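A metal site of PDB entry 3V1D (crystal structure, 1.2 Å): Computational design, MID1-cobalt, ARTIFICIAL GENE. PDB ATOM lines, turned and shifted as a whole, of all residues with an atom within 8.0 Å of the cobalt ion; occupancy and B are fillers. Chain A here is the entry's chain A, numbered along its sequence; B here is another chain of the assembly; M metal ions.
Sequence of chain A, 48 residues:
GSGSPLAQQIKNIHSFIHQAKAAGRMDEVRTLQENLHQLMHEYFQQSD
The cobalt ion is bound by NE2 of His 37 of chain B (2.1 Å), NE2 of His 41 of chain B (2.1 Å), NE2 of His 18 (2.2 Å) and NE2 of His 14 (2.2 Å). The cobalt ion has four donor atoms within binding distance.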
ATOM      1  N   LYS A  11       8.199   7.718  18.951  1.00  0.00           N
ATOM      2  CA  LYS A  11       7.072   7.679  18.053  1.00  0.00           C
ATOM      3  C   LYS A  11       7.495   7.167  16.673  1.00  0.00           C
ATOM      4  O   LYS A  11       6.808   6.359  16.059  1.00  0.00           O
ATOM      5  CB  LYS A  11       6.368   9.026  17.957  1.00  0.00           C
ATOM      6  CG  LYS A  11       5.612   9.396  19.197  1.00  0.00           C
ATOM      7  CD  LYS A  11       5.009  10.774  19.040  1.00  0.00           C
ATOM      8  CE  LYS A  11       4.204  11.163  20.249  1.00  0.00           C
ATOM      9  NZ  LYS A  11       3.830  12.571  20.136  1.00  0.00           N
ATOM     10  N   HIS A  14       8.378   3.350  16.748  1.00  0.00           N
ATOM     11  CA  HIS A  14       7.122   2.645  16.878  1.00  0.00           C
ATOM     12  C   HIS A  14       6.443   2.517  15.505  1.00  0.00           C
ATOM     13  O   HIS A  14       6.043   1.430  15.088  1.00  0.00           O
ATOM     14  CB  HIS A  14       6.303   3.426  17.888  1.00  0.00           C
ATOM     15  CG  HIS A  14       4.922   2.929  18.111  1.00  0.00           C
ATOM     16  ND1 HIS A  14       4.131   3.501  19.078  1.00  0.00           N
ATOM     17  CD2 HIS A  14       4.137   2.010  17.496  1.00  0.00           C
ATOM     18  CE1 HIS A  14       2.956   2.933  19.102  1.00  0.00           C
ATOM     19  NE2 HIS A  14       2.907   2.045  18.117  1.00  0.00           N
ATOM     20  N   SER A  15       6.327   3.615  14.769  1.00  0.00           N
ATOM     21  CA  SER A  15       5.708   3.553  13.461  1.00  0.00           C
ATOM     22  C   SER A  15       6.498   2.666  12.502  1.00  0.00           C
ATOM     23  O   SER A  15       5.933   1.908  11.696  1.00  0.00           O
ATOM     24  CB  SER A  15       5.584   4.944  12.879  1.00  0.00           C
ATOM     25  OG  SER A  15       5.060   4.866  11.559  1.00  0.00           O
ATOM     26  N   ILE A  17       8.228   0.080  13.209  1.00  0.00           N
ATOM     27  CA  ILE A  17       7.990  -1.345  13.529  1.00  0.00           C
ATOM     28  C   ILE A  17       6.740  -1.815  12.807  1.00  0.00           C
ATOM     29  O   ILE A  17       6.752  -2.891  12.189  1.00  0.00           O
ATOM     30  CB  ILE A  17       7.878  -1.565  15.057  1.00  0.00           C
ATOM     31  CG1 ILE A  17       9.252  -1.377  15.704  1.00  0.00           C
ATOM     32  CG2 ILE A  17       7.332  -2.953  15.362  1.00  0.00           C
ATOM     33  CD1 ILE A  17       9.165  -1.252  17.240  1.00  0.00           C
ATOM     34  N   HIS A  18       5.650  -1.052  12.861  1.00  0.00           N
ATOM     35  CA  HIS A  18       4.451  -1.476  12.147  1.00  0.00           C
ATOM     36  C   HIS A  18       4.707  -1.628  10.666  1.00  0.00           C
ATOM     37  O   HIS A  18       4.219  -2.581  10.036  1.00  0.00           O
ATOM     38  CB  HIS A  18       3.328  -0.470  12.361  1.00  0.00           C
ATOM     39  CG  HIS A  18       2.797  -0.434  13.755  1.00  0.00           C
ATOM     40  ND1 HIS A  18       2.246  -1.543  14.364  1.00  0.00           N
ATOM     41  CD2 HIS A  18       2.629   0.583  14.623  1.00  0.00           C
ATOM     42  CE1 HIS A  18       1.802  -1.210  15.573  1.00  0.00           C
ATOM     43  NE2 HIS A  18       2.003   0.074  15.732  1.00  0.00           N
ATOM     44  N   HIS B  37       2.721  -2.115  23.828  1.00  0.00           N
ATOM     45  CA  HIS B  37       2.259  -1.346  22.683  1.00  0.00           C
ATOM     46  C   HIS B  37       1.048  -0.487  23.021  1.00  0.00           C
ATOM     47  O   HIS B  37       0.986   0.703  22.698  1.00  0.00           O
ATOM     48  CB  HIS B  37       1.930  -2.317  21.540  1.00  0.00           C
ATOM     49  CG  HIS B  37       1.346  -1.640  20.325  1.00  0.00           C
ATOM     50  ND1 HIS B  37       0.064  -1.843  19.900  1.00  0.00           N
ATOM     51  CD2 HIS B  37       1.879  -0.718  19.494  1.00  0.00           C
ATOM     52  CE1 HIS B  37      -0.159  -1.101  18.828  1.00  0.00           C
ATOM     53  NE2 HIS B  37       0.931  -0.415  18.552  1.00  0.00           N
ATOM     54  N   GLN B  38       0.065  -1.089  23.669  1.00  0.00           N
ATOM     55  CA  GLN B  38      -1.118  -0.349  24.054  1.00  0.00           C
ATOM     56  C   GLN B  38      -0.747   0.789  24.995  1.00  0.00           C
ATOM     57  O   GLN B  38      -1.242   1.919  24.849  1.00  0.00           O
ATOM     58  CB  GLN B  38      -2.138  -1.270  24.730  1.00  0.00           C
ATOM     59  CG  GLN B  38      -3.359  -0.528  25.341  1.00  0.00           C
ATOM     60  CD  GLN B  38      -4.152   0.194  24.305  1.00  0.00           C
ATOM     61  OE1 GLN B  38      -4.188  -0.204  23.129  1.00  0.00           O
ATOM     62  NE2 GLN B  38      -4.821   1.277  24.734  1.00  0.00           N
ATOM     63  N   MET B  40       2.015   2.422  25.249  1.00  0.00           N
ATOM     64  CA  MET B  40       2.706   3.449  24.472  1.00  0.00           C
ATOM     65  C   MET B  40       1.715   4.312  23.724  1.00  0.00           C
ATOM     66  O   MET B  40       1.900   5.521  23.613  1.00  0.00           O
ATOM     67  CB  MET B  40       3.680   2.818  23.491  1.00  0.00           C
ATOM     68  CG  MET B  40       4.913   2.282  24.128  1.00  0.00           C
ATOM     69  SD  MET B  40       5.934   1.358  22.955  1.00  0.00           S
ATOM     70  CE  MET B  40       6.453   2.657  21.863  1.00  0.00           C
ATOM     71  N   HIS B  41       0.662   3.721  23.169  1.00  0.00           N
ATOM     72  CA  HIS B  41      -0.396   4.508  22.563  1.00  0.00           C
ATOM     73  C   HIS B  41      -1.078   5.450  23.551  1.00  0.00           C
ATOM     74  O   HIS B  41      -1.402   6.573  23.204  1.00  0.00           O
ATOM     75  CB  HIS B  41      -1.405   3.608  21.872  1.00  0.00           C
ATOM     76  CG  HIS B  41      -0.967   3.255  20.489  1.00  0.00           C
ATOM     77  ND1 HIS B  41      -1.070   4.142  19.450  1.00  0.00           N
ATOM     78  CD2 HIS B  41      -0.349   2.155  19.988  1.00  0.00           C
ATOM     79  CE1 HIS B  41      -0.592   3.584  18.348  1.00  0.00           C
ATOM     80  NE2 HIS B  41      -0.137   2.391  18.642  1.00  0.00           N
HETATM   81 CO    CO M   1       1.048   1.214  17.292  1.00  0.00          CO
